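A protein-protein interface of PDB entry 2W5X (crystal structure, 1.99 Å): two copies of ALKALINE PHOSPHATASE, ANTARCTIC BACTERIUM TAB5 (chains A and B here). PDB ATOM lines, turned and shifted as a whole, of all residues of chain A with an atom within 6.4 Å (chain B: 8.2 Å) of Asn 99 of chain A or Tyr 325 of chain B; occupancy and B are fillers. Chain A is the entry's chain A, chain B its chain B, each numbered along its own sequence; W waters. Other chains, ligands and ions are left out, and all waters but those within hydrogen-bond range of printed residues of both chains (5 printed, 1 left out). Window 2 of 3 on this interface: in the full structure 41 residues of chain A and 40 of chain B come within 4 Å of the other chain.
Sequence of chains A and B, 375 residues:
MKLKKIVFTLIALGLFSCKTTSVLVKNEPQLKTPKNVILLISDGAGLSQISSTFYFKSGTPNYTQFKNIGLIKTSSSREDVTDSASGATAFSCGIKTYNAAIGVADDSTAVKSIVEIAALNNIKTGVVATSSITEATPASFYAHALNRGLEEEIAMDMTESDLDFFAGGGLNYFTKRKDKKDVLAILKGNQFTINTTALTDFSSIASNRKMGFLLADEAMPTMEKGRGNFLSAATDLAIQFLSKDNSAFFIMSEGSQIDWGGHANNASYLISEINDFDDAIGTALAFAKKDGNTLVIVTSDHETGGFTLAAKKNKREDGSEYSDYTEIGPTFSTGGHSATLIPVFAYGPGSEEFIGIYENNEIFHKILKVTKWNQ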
ATOM      1  N   SER A  75       6.269  -9.958 -13.105  1.00  0.00           N
ATOM      2  CA  SER A  75       5.337  -9.544 -14.154  1.00  0.00           C
ATOM      3  C   SER A  75       3.895  -9.444 -13.617  1.00  0.00           C
ATOM      4  O   SER A  75       3.489 -10.229 -12.761  1.00  0.00           O
ATOM      5  CB  SER A  75       5.407 -10.511 -15.346  1.00  0.00           C
ATOM      6  OG  SER A  75       6.696 -10.475 -15.958  1.00  0.00           O
ATOM      7  N   SER A  76       3.131  -8.476 -14.116  1.00  0.00           N
ATOM      8  CA  SER A  76       1.747  -8.310 -13.675  1.00  0.00           C
ATOM      9  C   SER A  76       0.830  -9.237 -14.473  1.00  0.00           C
ATOM     10  O   SER A  76       1.300 -10.045 -15.263  1.00  0.00           O
ATOM     11  CB  SER A  76       1.298  -6.859 -13.852  1.00  0.00           C
ATOM     12  OG  SER A  76       0.988  -6.606 -15.211  1.00  0.00           O
ATOM     13  N   SER A  77      -0.478  -9.119 -14.273  1.00  0.00           N
ATOM     14  CA  SER A  77      -1.419  -9.956 -15.010  1.00  0.00           C
ATOM     15  C   SER A  77      -1.457  -9.615 -16.499  1.00  0.00           C
ATOM     16  O   SER A  77      -1.916 -10.423 -17.294  1.00  0.00           O
ATOM     17  CB  SER A  77      -2.834  -9.846 -14.418  1.00  0.00           C
ATOM     18  OG  SER A  77      -3.331  -8.524 -14.566  1.00  0.00           O
ATOM     19  N   ARG A  78      -0.991  -8.424 -16.878  1.00  0.00           N
ATOM     20  CA  ARG A  78      -1.102  -7.979 -18.277  1.00  0.00           C
ATOM     21  C   ARG A  78       0.213  -7.495 -18.870  1.00  0.00           C
ATOM     22  O   ARG A  78       0.308  -7.305 -20.075  1.00  0.00           O
ATOM     23  CB  ARG A  78      -2.135  -6.850 -18.434  1.00  0.00           C
ATOM     24  CG  ARG A  78      -3.505  -7.145 -17.852  1.00  0.00           C
ATOM     25  CD  ARG A  78      -4.551  -6.107 -18.279  1.00  0.00           C
ATOM     26  NE  ARG A  78      -5.804  -6.313 -17.548  1.00  0.00           N
ATOM     27  CZ  ARG A  78      -6.939  -5.660 -17.788  1.00  0.00           C
ATOM     28  NH1 ARG A  78      -6.997  -4.750 -18.750  1.00  0.00           N
ATOM     29  NH2 ARG A  78      -8.024  -5.922 -17.067  1.00  0.00           N
ATOM     30  N   GLU A  79       1.215  -7.267 -18.026  1.00  0.00           N
ATOM     31  CA  GLU A  79       2.450  -6.633 -18.476  1.00  0.00           C
ATOM     32  C   GLU A  79       3.693  -7.389 -18.001  1.00  0.00           C
ATOM     33  O   GLU A  79       3.797  -7.749 -16.823  1.00  0.00           O
ATOM     34  CB  GLU A  79       2.488  -5.168 -18.002  1.00  0.00           C
ATOM     35  CG  GLU A  79       1.361  -4.265 -18.584  1.00  0.00           C
ATOM     36  CD  GLU A  79       0.197  -3.989 -17.608  1.00  0.00           C
ATOM     37  OE1 GLU A  79       0.163  -4.565 -16.496  1.00  0.00           O
ATOM     38  OE2 GLU A  79      -0.690  -3.179 -17.959  1.00  0.00           O
ATOM     39  N   ASP A  80       4.626  -7.646 -18.915  1.00  0.00           N
ATOM     40  CA  ASP A  80       5.896  -8.284 -18.552  1.00  0.00           C
ATOM     41  C   ASP A  80       6.645  -7.429 -17.526  1.00  0.00           C
ATOM     42  O   ASP A  80       7.297  -7.950 -16.612  1.00  0.00           O
ATOM     43  CB  ASP A  80       6.781  -8.507 -19.789  1.00  0.00           C
ATOM     44  CG  ASP A  80       6.376  -9.732 -20.594  1.00  0.00           C
ATOM     45  OD1 ASP A  80       5.604 -10.567 -20.079  1.00  0.00           O
ATOM     46  OD2 ASP A  80       6.841  -9.870 -21.745  1.00  0.00           O
ATOM     47  N   VAL A  81       6.543  -6.113 -17.694  1.00  0.00           N
ATOM     48  CA  VAL A  81       7.174  -5.157 -16.788  1.00  0.00           C
ATOM     49  C   VAL A  81       6.113  -4.520 -15.877  1.00  0.00           C
ATOM     50  O   VAL A  81       5.231  -3.793 -16.329  1.00  0.00           O
ATOM     51  CB  VAL A  81       7.952  -4.071 -17.573  1.00  0.00           C
ATOM     52  CG1 VAL A  81       8.666  -3.109 -16.625  1.00  0.00           C
ATOM     53  CG2 VAL A  81       8.968  -4.732 -18.515  1.00  0.00           C
ATOM     54  N   THR A  82       6.219  -4.803 -14.586  1.00  0.00           N
ATOM     55  CA  THR A  82       5.250  -4.351 -13.604  1.00  0.00           C
ATOM     56  C   THR A  82       5.459  -2.894 -13.180  1.00  0.00           C
ATOM     57  O   THR A  82       6.543  -2.336 -13.340  1.00  0.00           O
ATOM     58  CB  THR A  82       5.325  -5.253 -12.346  1.00  0.00           C
ATOM     59  OG1 THR A  82       4.221  -4.973 -11.473  1.00  0.00           O
ATOM     60  CG2 THR A  82       6.655  -5.033 -11.606  1.00  0.00           C
ATOM     61  N   ASP A  83       4.413  -2.277 -12.640  1.00  0.00           N
ATOM     62  CA  ASP A  83       4.579  -1.010 -11.936  1.00  0.00           C
ATOM     63  C   ASP A  83       4.434  -1.277 -10.435  1.00  0.00           C
ATOM     64  O   ASP A  83       4.198  -2.414 -10.028  1.00  0.00           O
ATOM     65  CB  ASP A  83       3.590   0.061 -12.436  1.00  0.00           C
ATOM     66  CG  ASP A  83       2.245   0.004 -11.722  1.00  0.00           C
ATOM     67  OD1 ASP A  83       1.781  -1.110 -11.407  1.00  0.00           O
ATOM     68  OD2 ASP A  83       1.653   1.076 -11.482  1.00  0.00           O
ATOM     69  N   SEP A  84       4.591  -0.238  -9.623  1.00  0.00           N
ATOM     70  CA  SEP A  84       4.597  -0.380  -8.168  1.00  0.00           C
ATOM     71  CB  SEP A  84       5.092   0.927  -7.510  1.00  0.00           C
ATOM     72  OG  SEP A  84       6.355   1.324  -8.020  1.00  0.00           O
ATOM     73  C   SEP A  84       3.220  -0.795  -7.607  1.00  0.00           C
ATOM     74  O   SEP A  84       3.131  -1.382  -6.528  1.00  0.00           O
ATOM     75  P   SEP A  84       6.468   2.711  -8.874  1.00  0.00           P
ATOM     76  O1P SEP A  84       5.819   3.947  -8.078  1.00  0.00           O
ATOM     77  O2P SEP A  84       5.748   2.581 -10.312  1.00  0.00           O
ATOM     78  O3P SEP A  84       8.031   2.994  -9.026  1.00  0.00           O
ATOM     79  N   ALA A  85       2.147  -0.505  -8.344  1.00  0.00           N
ATOM     80  CA  ALA A  85       0.796  -0.769  -7.841  1.00  0.00           C
ATOM     81  C   ALA A  85       0.425  -2.245  -7.928  1.00  0.00           C
ATOM     82  O   ALA A  85       0.028  -2.861  -6.934  1.00  0.00           O
ATOM     83  CB  ALA A  85      -0.232   0.082  -8.584  1.00  0.00           C
ATOM     84  N   SER A  86       0.548  -2.820  -9.118  1.00  0.00           N
ATOM     85  CA  SER A  86       0.271  -4.245  -9.266  1.00  0.00           C
ATOM     86  C   SER A  86       1.323  -5.069  -8.520  1.00  0.00           C
ATOM     87  O   SER A  86       1.018  -6.137  -7.979  1.00  0.00           O
ATOM     88  CB  SER A  86       0.215  -4.647 -10.742  1.00  0.00           C
ATOM     89  OG  SER A  86       1.452  -4.419 -11.388  1.00  0.00           O
ATOM     90  N   GLY A  87       2.556  -4.567  -8.496  1.00  0.00           N
ATOM     91  CA  GLY A  87       3.656  -5.251  -7.832  1.00  0.00           C
ATOM     92  C   GLY A  87       3.426  -5.394  -6.335  1.00  0.00           C
ATOM     93  O   GLY A  87       3.748  -6.417  -5.745  1.00  0.00           O
ATOM     94  N   THR A  97      -2.376  -8.677 -10.914  1.00  0.00           N
ATOM     95  CA  THR A  97      -3.343  -7.677 -11.349  1.00  0.00           C
ATOM     96  C   THR A  97      -2.713  -6.698 -12.343  1.00  0.00           C
ATOM     97  O   THR A  97      -1.514  -6.775 -12.616  1.00  0.00           O
ATOM     98  CB  THR A  97      -3.969  -6.937 -10.148  1.00  0.00           C
ATOM     99  OG1 THR A  97      -5.143  -6.237 -10.576  1.00  0.00           O
ATOM    100  CG2 THR A  97      -2.970  -5.964  -9.522  1.00  0.00           C
ATOM    101  N   TYR A  98      -3.520  -5.793 -12.889  1.00  0.00           N
ATOM    102  CA  TYR A  98      -3.042  -4.886 -13.925  1.00  0.00           C
ATOM    103  C   TYR A  98      -2.217  -3.745 -13.330  1.00  0.00           C
ATOM    104  O   TYR A  98      -2.487  -3.295 -12.214  1.00  0.00           O
ATOM    105  CB  TYR A  98      -4.214  -4.355 -14.772  1.00  0.00           C
ATOM    106  CG  TYR A  98      -5.265  -3.610 -13.972  1.00  0.00           C
ATOM    107  CD1 TYR A  98      -5.122  -2.255 -13.695  1.00  0.00           C
ATOM    108  CD2 TYR A  98      -6.389  -4.263 -13.479  1.00  0.00           C
ATOM    109  CE1 TYR A  98      -6.073  -1.569 -12.955  1.00  0.00           C
ATOM    110  CE2 TYR A  98      -7.347  -3.581 -12.735  1.00  0.00           C
ATOM    111  CZ  TYR A  98      -7.179  -2.236 -12.479  1.00  0.00           C
ATOM    112  OH  TYR A  98      -8.115  -1.547 -11.745  1.00  0.00           O
ATOM    113  N   ASN A  99      -1.188  -3.311 -14.064  1.00  0.00           N
ATOM    114  CA  ASN A  99      -0.409  -2.137 -13.684  1.00  0.00           C
ATOM    115  C   ASN A  99      -1.343  -0.974 -13.365  1.00  0.00           C
ATOM    116  O   ASN A  99      -2.244  -0.662 -14.153  1.00  0.00           O
ATOM    117  CB  ASN A  99       0.561  -1.731 -14.805  1.00  0.00           C
ATOM    118  CG  ASN A  99       1.786  -2.634 -14.881  1.00  0.00           C
ATOM    119  OD1 ASN A  99       1.922  -3.586 -14.108  1.00  0.00           O
ATOM    120  ND2 ASN A  99       2.692  -2.334 -15.813  1.00  0.00           N
ATOM    121  N   ALA A 100      -1.121  -0.359 -12.204  1.00  0.00           N
ATOM    122  CA  ALA A 100      -1.920   0.757 -11.682  1.00  0.00           C
ATOM    123  C   ALA A 100      -3.010   0.341 -10.689  1.00  0.00           C
ATOM    124  O   ALA A 100      -3.562   1.186  -9.984  1.00  0.00           O
ATOM    125  CB  ALA A 100      -2.518   1.618 -12.808  1.00  0.00           C
ATOM    126  N   ALA A 101      -3.316  -0.946 -10.622  1.00  0.00           N
ATOM    127  CA  ALA A 101      -4.364  -1.409  -9.709  1.00  0.00           C
ATOM    128  C   ALA A 101      -3.912  -1.342  -8.253  1.00  0.00           C
ATOM    129  O   ALA A 101      -2.761  -1.636  -7.941  1.00  0.00           O
ATOM    130  CB  ALA A 101      -4.794  -2.824 -10.058  1.00  0.00           C
ATOM    131  N   LEU A 146      -9.331   1.710  -8.279  1.00  0.00           N
ATOM    132  CA  LEU A 146      -9.156   1.215  -9.636  1.00  0.00           C
ATOM    133  C   LEU A 146      -7.847   1.698 -10.255  1.00  0.00           C
ATOM    134  O   LEU A 146      -7.328   1.075 -11.178  1.00  0.00           O
ATOM    135  CB  LEU A 146     -10.337   1.623 -10.526  1.00  0.00           C
ATOM    136  CG  LEU A 146     -11.715   1.059 -10.166  1.00  0.00           C
ATOM    137  CD1 LEU A 146     -12.744   1.502 -11.188  1.00  0.00           C
ATOM    138  CD2 LEU A 146     -11.686  -0.456 -10.075  1.00  0.00           C
ATOM    139  N   ASN A 147      -7.329   2.816  -9.753  1.00  0.00           N
ATOM    140  CA  ASN A 147      -6.097   3.394 -10.282  1.00  0.00           C
ATOM    141  C   ASN A 147      -5.291   4.093  -9.198  1.00  0.00           C
ATOM    142  O   ASN A 147      -5.834   4.846  -8.388  1.00  0.00           O
ATOM    143  CB  ASN A 147      -6.393   4.370 -11.423  1.00  0.00           C
ATOM    144  CG  ASN A 147      -5.135   4.815 -12.152  1.00  0.00           C
ATOM    145  OD1 ASN A 147      -4.344   5.593 -11.628  1.00  0.00           O
ATOM    146  ND2 ASN A 147      -4.949   4.320 -13.368  1.00  0.00           N
ATOM    147  N   ARG A 148      -3.988   3.842  -9.196  1.00  0.00           N
ATOM    148  CA  ARG A 148      -3.080   4.359  -8.174  1.00  0.00           C
ATOM    149  C   ARG A 148      -3.060   5.889  -8.068  1.00  0.00           C
ATOM    150  O   ARG A 148      -2.677   6.433  -7.037  1.00  0.00           O
ATOM    151  CB  ARG A 148      -1.666   3.881  -8.487  1.00  0.00           C
ATOM    152  CG  ARG A 148      -1.150   4.410  -9.827  1.00  0.00           C
ATOM    153  CD  ARG A 148       0.243   3.895 -10.103  1.00  0.00           C
ATOM    154  NE  ARG A 148       1.224   4.446  -9.172  1.00  0.00           N
ATOM    155  CZ  ARG A 148       2.506   4.081  -9.136  1.00  0.00           C
ATOM    156  NH1 ARG A 148       2.955   3.152  -9.968  1.00  0.00           N
ATOM    157  NH2 ARG A 148       3.339   4.646  -8.272  1.00  0.00           N
ATOM    158  N   HIS A 263      14.887   5.977 -11.474  1.00  0.00           N
ATOM    159  CA  HIS A 263      14.272   6.719 -12.573  1.00  0.00           C
ATOM    160  C   HIS A 263      15.098   7.924 -12.974  1.00  0.00           C
ATOM    161  O   HIS A 263      15.176   8.266 -14.151  1.00  0.00           O
ATOM    162  CB  HIS A 263      12.876   7.200 -12.192  1.00  0.00           C
ATOM    163  CG  HIS A 263      11.840   6.125 -12.227  1.00  0.00           C
ATOM    164  ND1 HIS A 263      11.529   5.431 -13.376  1.00  0.00           N
ATOM    165  CD2 HIS A 263      11.036   5.630 -11.257  1.00  0.00           C
ATOM    166  CE1 HIS A 263      10.576   4.554 -13.113  1.00  0.00           C
ATOM    167  NE2 HIS A 263      10.258   4.658 -11.836  1.00  0.00           N
ATOM    168  N   GLY A 335      15.250   4.491 -18.106  1.00  0.00           N
ATOM    169  CA  GLY A 335      14.612   5.422 -17.193  1.00  0.00           C
ATOM    170  C   GLY A 335      13.426   4.786 -16.490  1.00  0.00           C
ATOM    171  O   GLY A 335      12.811   5.394 -15.620  1.00  0.00           O
ATOM    172  N   GLY A 336      13.101   3.553 -16.861  1.00  0.00           N
ATOM    173  CA  GLY A 336      11.945   2.878 -16.288  1.00  0.00           C
ATOM    174  C   GLY A 336      12.307   1.606 -15.534  1.00  0.00           C
ATOM    175  O   GLY A 336      13.472   1.386 -15.190  1.00  0.00           O
ATOM    176  N   HIS A 337      11.296   0.777 -15.280  1.00  0.00           N
ATOM    177  CA  HIS A 337      11.451  -0.489 -14.574  1.00  0.00           C
ATOM    178  C   HIS A 337      12.031  -1.562 -15.481  1.00  0.00           C
ATOM    179  O   HIS A 337      12.075  -1.394 -16.697  1.00  0.00           O
ATOM    180  CB  HIS A 337      10.087  -0.978 -14.072  1.00  0.00           C
ATOM    181  CG  HIS A 337       9.421  -0.043 -13.108  1.00  0.00           C
ATOM    182  ND1 HIS A 337       8.118  -0.210 -12.695  1.00  0.00           N
ATOM    183  CD2 HIS A 337       9.874   1.072 -12.484  1.00  0.00           C
ATOM    184  CE1 HIS A 337       7.795   0.757 -11.852  1.00  0.00           C
ATOM    185  NE2 HIS A 337       8.841   1.551 -11.711  1.00  0.00           N
ATOM    186  N   SER A 338      12.469  -2.673 -14.888  1.00  0.00           N
ATOM    187  CA  SER A 338      12.870  -3.843 -15.673  1.00  0.00           C
ATOM    188  C   SER A 338      12.311  -5.134 -15.068  1.00  0.00           C
ATOM    189  O   SER A 338      11.876  -5.153 -13.918  1.00  0.00           O
ATOM    190  CB  SER A 338      14.397  -3.932 -15.811  1.00  0.00           C
ATOM    191  OG  SER A 338      15.002  -4.290 -14.580  1.00  0.00           O
ATOM    192  N   LEU B 309      16.402  -6.213 -18.447  1.00  0.00           N
ATOM    193  CA  LEU B 309      15.145  -6.570 -19.105  1.00  0.00           C
ATOM    194  C   LEU B 309      14.195  -5.379 -19.086  1.00  0.00           C
ATOM    195  O   LEU B 309      13.124  -5.407 -18.459  1.00  0.00           O
ATOM    196  CB  LEU B 309      14.514  -7.800 -18.447  1.00  0.00           C
ATOM    197  CG  LEU B 309      15.365  -9.070 -18.569  1.00  0.00           C
ATOM    198  CD1 LEU B 309      14.722 -10.231 -17.832  1.00  0.00           C
ATOM    199  CD2 LEU B 309      15.576  -9.415 -20.036  1.00  0.00           C
ATOM    200  N   ALA B 310      14.613  -4.330 -19.776  1.00  0.00           N
ATOM    201  CA  ALA B 310      13.884  -3.067 -19.828  1.00  0.00           C
ATOM    202  C   ALA B 310      12.600  -3.196 -20.630  1.00  0.00           C
ATOM    203  O   ALA B 310      12.405  -4.175 -21.347  1.00  0.00           O
ATOM    204  CB  ALA B 310      14.766  -1.979 -20.428  1.00  0.00           C
ATOM    205  N   ALA B 311      11.736  -2.192 -20.509  1.00  0.00           N
ATOM    206  CA  ALA B 311      10.502  -2.138 -21.283  1.00  0.00           C
ATOM    207  C   ALA B 311      10.822  -1.897 -22.750  1.00  0.00           C
ATOM    208  O   ALA B 311      11.758  -1.168 -23.077  1.00  0.00           O
ATOM    209  CB  ALA B 311       9.598  -1.041 -20.763  1.00  0.00           C
ATOM    210  N   LYS B 312      10.042  -2.514 -23.631  1.00  0.00           N
ATOM    211  CA  LYS B 312      10.213  -2.324 -25.063  1.00  0.00           C
ATOM    212  C   LYS B 312       9.933  -0.868 -25.408  1.00  0.00           C
ATOM    213  O   LYS B 312       8.985  -0.273 -24.901  1.00  0.00           O
ATOM    214  CB  LYS B 312       9.257  -3.236 -25.832  1.00  0.00           C
ATOM    215  CG  LYS B 312       9.759  -3.671 -27.197  1.00  0.00           C
ATOM    216  CD  LYS B 312       8.893  -4.794 -27.744  1.00  0.00           C
ATOM    217  CE  LYS B 312       9.590  -5.553 -28.862  1.00  0.00           C
ATOM    218  NZ  LYS B 312       8.925  -6.863 -29.132  1.00  0.00           N
ATOM    219  N   LYS B 313      10.763  -0.298 -26.272  1.00  0.00           N
ATOM    220  CA  LYS B 313      10.624   1.095 -26.657  1.00  0.00           C
ATOM    221  C   LYS B 313       9.734   1.208 -27.891  1.00  0.00           C
ATOM    222  O   LYS B 313      10.090   0.718 -28.958  1.00  0.00           O
ATOM    223  CB  LYS B 313      11.999   1.696 -26.948  1.00  0.00           C
ATOM    224  CG  LYS B 313      12.241   3.049 -26.311  1.00  0.00           C
ATOM    225  CD  LYS B 313      12.804   2.905 -24.907  1.00  0.00           C
ATOM    226  CE  LYS B 313      12.764   4.226 -24.152  1.00  0.00           C
ATOM    227  NZ  LYS B 313      13.573   5.284 -24.816  1.00  0.00           N
ATOM    228  N   ASN B 314       8.572   1.837 -27.734  1.00  0.00           N
ATOM    229  CA  ASN B 314       7.666   2.085 -28.854  1.00  0.00           C
ATOM    230  C   ASN B 314       7.878   3.460 -29.477  1.00  0.00           C
ATOM    231  O   ASN B 314       8.503   4.338 -28.878  1.00  0.00           O
ATOM    232  CB  ASN B 314       6.206   1.928 -28.427  1.00  0.00           C
ATOM    233  CG  ASN B 314       5.740   0.489 -28.462  1.00  0.00           C
ATOM    234  OD1 ASN B 314       6.488  -0.408 -28.849  1.00  0.00           O
ATOM    235  ND2 ASN B 314       4.491   0.262 -28.062  1.00  0.00           N
ATOM    236  N   TYR B 322       8.535   6.171 -26.591  1.00  0.00           N
ATOM    237  CA  TYR B 322       7.922   5.936 -25.286  1.00  0.00           C
ATOM    238  C   TYR B 322       8.040   4.472 -24.846  1.00  0.00           C
ATOM    239  O   TYR B 322       8.234   3.581 -25.671  1.00  0.00           O
ATOM    240  CB  TYR B 322       6.456   6.377 -25.288  1.00  0.00           C
ATOM    241  CG  TYR B 322       5.529   5.453 -26.043  1.00  0.00           C
ATOM    242  CD1 TYR B 322       4.827   4.452 -25.381  1.00  0.00           C
ATOM    243  CD2 TYR B 322       5.345   5.586 -27.413  1.00  0.00           C
ATOM    244  CE1 TYR B 322       3.975   3.607 -26.062  1.00  0.00           C
ATOM    245  CE2 TYR B 322       4.493   4.743 -28.105  1.00  0.00           C
ATOM    246  CZ  TYR B 322       3.811   3.755 -27.423  1.00  0.00           C
ATOM    247  OH  TYR B 322       2.965   2.910 -28.101  1.00  0.00           O
ATOM    248  N   SER B 323       7.917   4.237 -23.544  1.00  0.00           N
ATOM    249  CA  SER B 323       8.087   2.901 -22.978  1.00  0.00           C
ATOM    250  C   SER B 323       6.784   2.114 -22.947  1.00  0.00           C
ATOM    251  O   SER B 323       5.738   2.634 -22.562  1.00  0.00           O
ATOM    252  CB  SER B 323       8.669   2.987 -21.565  1.00  0.00           C
ATOM    253  OG  SER B 323       9.942   3.598 -21.589  1.00  0.00           O
ATOM    254  N   ASP B 324       6.857   0.852 -23.352  1.00  0.00           N
ATOM    255  CA  ASP B 324       5.690  -0.019 -23.354  1.00  0.00           C
ATOM    256  C   ASP B 324       5.945  -1.211 -22.440  1.00  0.00           C
ATOM    257  O   ASP B 324       6.636  -2.157 -22.813  1.00  0.00           O
ATOM    258  CB  ASP B 324       5.364  -0.484 -24.774  1.00  0.00           C
ATOM    259  CG  ASP B 324       4.164  -1.412 -24.822  1.00  0.00           C
ATOM    260  OD1 ASP B 324       3.557  -1.674 -23.759  1.00  0.00           O
ATOM    261  OD2 ASP B 324       3.828  -1.882 -25.927  1.00  0.00           O
ATOM    262  N   TYR B 325       5.378  -1.146 -21.241  1.00  0.00           N
ATOM    263  CA  TYR B 325       5.614  -2.136 -20.198  1.00  0.00           C
ATOM    264  C   TYR B 325       5.026  -3.514 -20.496  1.00  0.00           C
ATOM    265  O   TYR B 325       5.261  -4.457 -19.744  1.00  0.00           O
ATOM    266  CB  TYR B 325       5.093  -1.613 -18.851  1.00  0.00           C
ATOM    267  CG  TYR B 325       6.051  -0.681 -18.127  1.00  0.00           C
ATOM    268  CD1 TYR B 325       6.977   0.085 -18.829  1.00  0.00           C
ATOM    269  CD2 TYR B 325       6.021  -0.564 -16.740  1.00  0.00           C
ATOM    270  CE1 TYR B 325       7.850   0.935 -18.172  1.00  0.00           C
ATOM    271  CE2 TYR B 325       6.886   0.286 -16.072  1.00  0.00           C
ATOM    272  CZ  TYR B 325       7.799   1.027 -16.791  1.00  0.00           C
ATOM    273  OH  TYR B 325       8.658   1.868 -16.126  1.00  0.00           O
ATOM    274  N   THR B 326       4.268  -3.643 -21.583  1.00  0.00           N
ATOM    275  CA  THR B 326       3.710  -4.952 -21.925  1.00  0.00           C
ATOM    276  C   THR B 326       4.806  -5.943 -22.304  1.00  0.00           C
ATOM    277  O   THR B 326       4.723  -7.122 -21.973  1.00  0.00           O
ATOM    278  CB  THR B 326       2.686  -4.882 -23.077  1.00  0.00           C
ATOM    279  OG1 THR B 326       3.258  -4.166 -24.174  1.00  0.00           O
ATOM    280  CG2 THR B 326       1.430  -4.172 -22.625  1.00  0.00           C
ATOM    281  N   GLU B 327       5.834  -5.460 -22.993  1.00  0.00           N
ATOM    282  CA  GLU B 327       6.921  -6.322 -23.453  1.00  0.00           C
ATOM    283  C   GLU B 327       8.302  -5.830 -23.038  1.00  0.00           C
ATOM    284  O   GLU B 327       8.470  -4.691 -22.594  1.00  0.00           O
ATOM    285  CB  GLU B 327       6.893  -6.463 -24.975  1.00  0.00           C
ATOM    286  CG  GLU B 327       5.684  -7.207 -25.512  1.00  0.00           C
ATOM    287  CD  GLU B 327       5.756  -7.401 -27.011  1.00  0.00           C
ATOM    288  OE1 GLU B 327       4.826  -6.958 -27.714  1.00  0.00           O
ATOM    289  OE2 GLU B 327       6.754  -7.981 -27.489  1.00  0.00           O
ATOM    290  N   ILE B 328       9.291  -6.699 -23.225  1.00  0.00           N
ATOM    291  CA  ILE B 328      10.667  -6.435 -22.820  1.00  0.00           C
ATOM    292  C   ILE B 328      11.561  -6.144 -24.024  1.00  0.00           C
ATOM    293  O   ILE B 328      11.491  -6.837 -25.033  1.00  0.00           O
ATOM    294  CB  ILE B 328      11.248  -7.653 -22.077  1.00  0.00           C
ATOM    295  CG1 ILE B 328      10.502  -7.875 -20.756  1.00  0.00           C
ATOM    296  CG2 ILE B 328      12.739  -7.470 -21.840  1.00  0.00           C
ATOM    297  CD1 ILE B 328      10.695  -9.267 -20.159  1.00  0.00           C
HETATM  298  O   HOH W   1      16.765  -6.221 -15.569  1.00  0.00           O
HETATM  299  O   HOH W   2      11.109   3.330 -19.432  1.00  0.00           O
HETATM  300  O   HOH W   3      12.336   0.288 -18.792  1.00  0.00           O
HETATM  301  O   HOH W   4       2.376  -9.142 -22.026  1.00  0.00           O
HETATM  302  O   HOH W   5       8.908  -9.901 -23.725  1.00  0.00           O
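The backbone NH (N) of Asp 80 of chain A sits at hydrogen-bond distance from the backbone carbonyl oxygen (O) of Tyr 325 of chain B (3.4 Å). The backbone NH (N) of Asp 80 of chain A is in hydrogen-bond range of the backbone carbonyl oxygen (O) of Thr 326 of chain B, at 3.1 Å. O of Tyr 325 of chain B lies within hydrogen-bond range of N of Val 81 of chain A, at 2.9 Å. The side-chain hydroxyl of Tyr 325 of chain B sits at hydrogen-bond distance from the backbone NH of His 337 of chain A (3.0 Å).
The side-chain carboxylate of Glu 79 of chain A lies within hydrogen-bond range of the side-chain hydroxyl of Ser 76 of chain A (2.5 Å). OG1 of Thr 82 of chain A lies within hydrogen-bond range of OG of Ser 86 of chain A, 2.8 Å away. OG of Ser 86 of chain A is in hydrogen-bond range of OD1 of Asn 99 of chain A (2.9 Å).
Tyr 325 of chain B touches Glu 79 of chain A (O to CB, 3.4 Å). Ile 328 of chain B touches Asp 80 of chain A (CG1 to CB, 3.9 Å). Thr 82 of chain A touches Tyr 325 of chain B (O to CE2, 3.8 Å). His 337 of chain A touches Ala 311 of chain B (O to N, 3.9 Å). Ser 338 of chain A touches Leu 309 of chain B. Ser 338 of chain A touches Ala 310 of chain B.
Of chain A, only Glu 79 (3.4 Å), Asp 80 (3.4 Å), Val 81 (2.9 Å), Thr 82 (3.8 Å), Asn 99 (3.9 Å), Gly 336 (3.4 Å) and His 337 (3.0 Å) come within 4 Å of Tyr 325 of chain B. Val 81 of chain A touches one residue of chain B. Of the printed residues of chain A, Ala 310 of chain B touches His 337 (3.98 Å) and Ser 338 (3.99 Å). Printed residues of chain A within 4 Å of Thr 326 of chain B: Asp 80. The nearest residue of chain B that does not touch Asn 99 of chain A is Thr 326 of chain B (6.1 Å). The nearest residue of chain A that does not touch Tyr 325 of chain B is His 263 of chain A (4.5 Å). The nearest printed residue of chain A that does not touch Ala 311 of chain B is Val 81 of chain A (4.1 Å).
Of the 13 printed residues of chain B, 7 touch a printed residue of chain A. Printed residues of chain B that touch a printed residue of chain A: Leu 309, Ala 310, Ala 311, Tyr 325, Thr 326, Glu 327 and Ile 328. Hydrophobic or aromatic side chains of chain B that line the printed part of chain A: Tyr 325 and Ile 328. Of the 26 printed residues of chain A, 8 touch a printed residue of chain B. Among the printed residues, 14 pairs touch across the chains.
No position is printed for both chains. Of the 14 pairs that touch across the chains among the printed residues, none has its exchanged pair printed and touching as well.
Water W3 bridges the backbone carbonyl oxygen of His 337 of chain A (2.7 Å) and the backbone NH of Ala 311 of chain B (3.1 Å). Water W1 lies within hydrogen-bond range of the side-chain hydroxyl of Ser 338 of chain A (2.8 Å) and the backbone NH of Leu 309 of chain B (2.9 Å).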
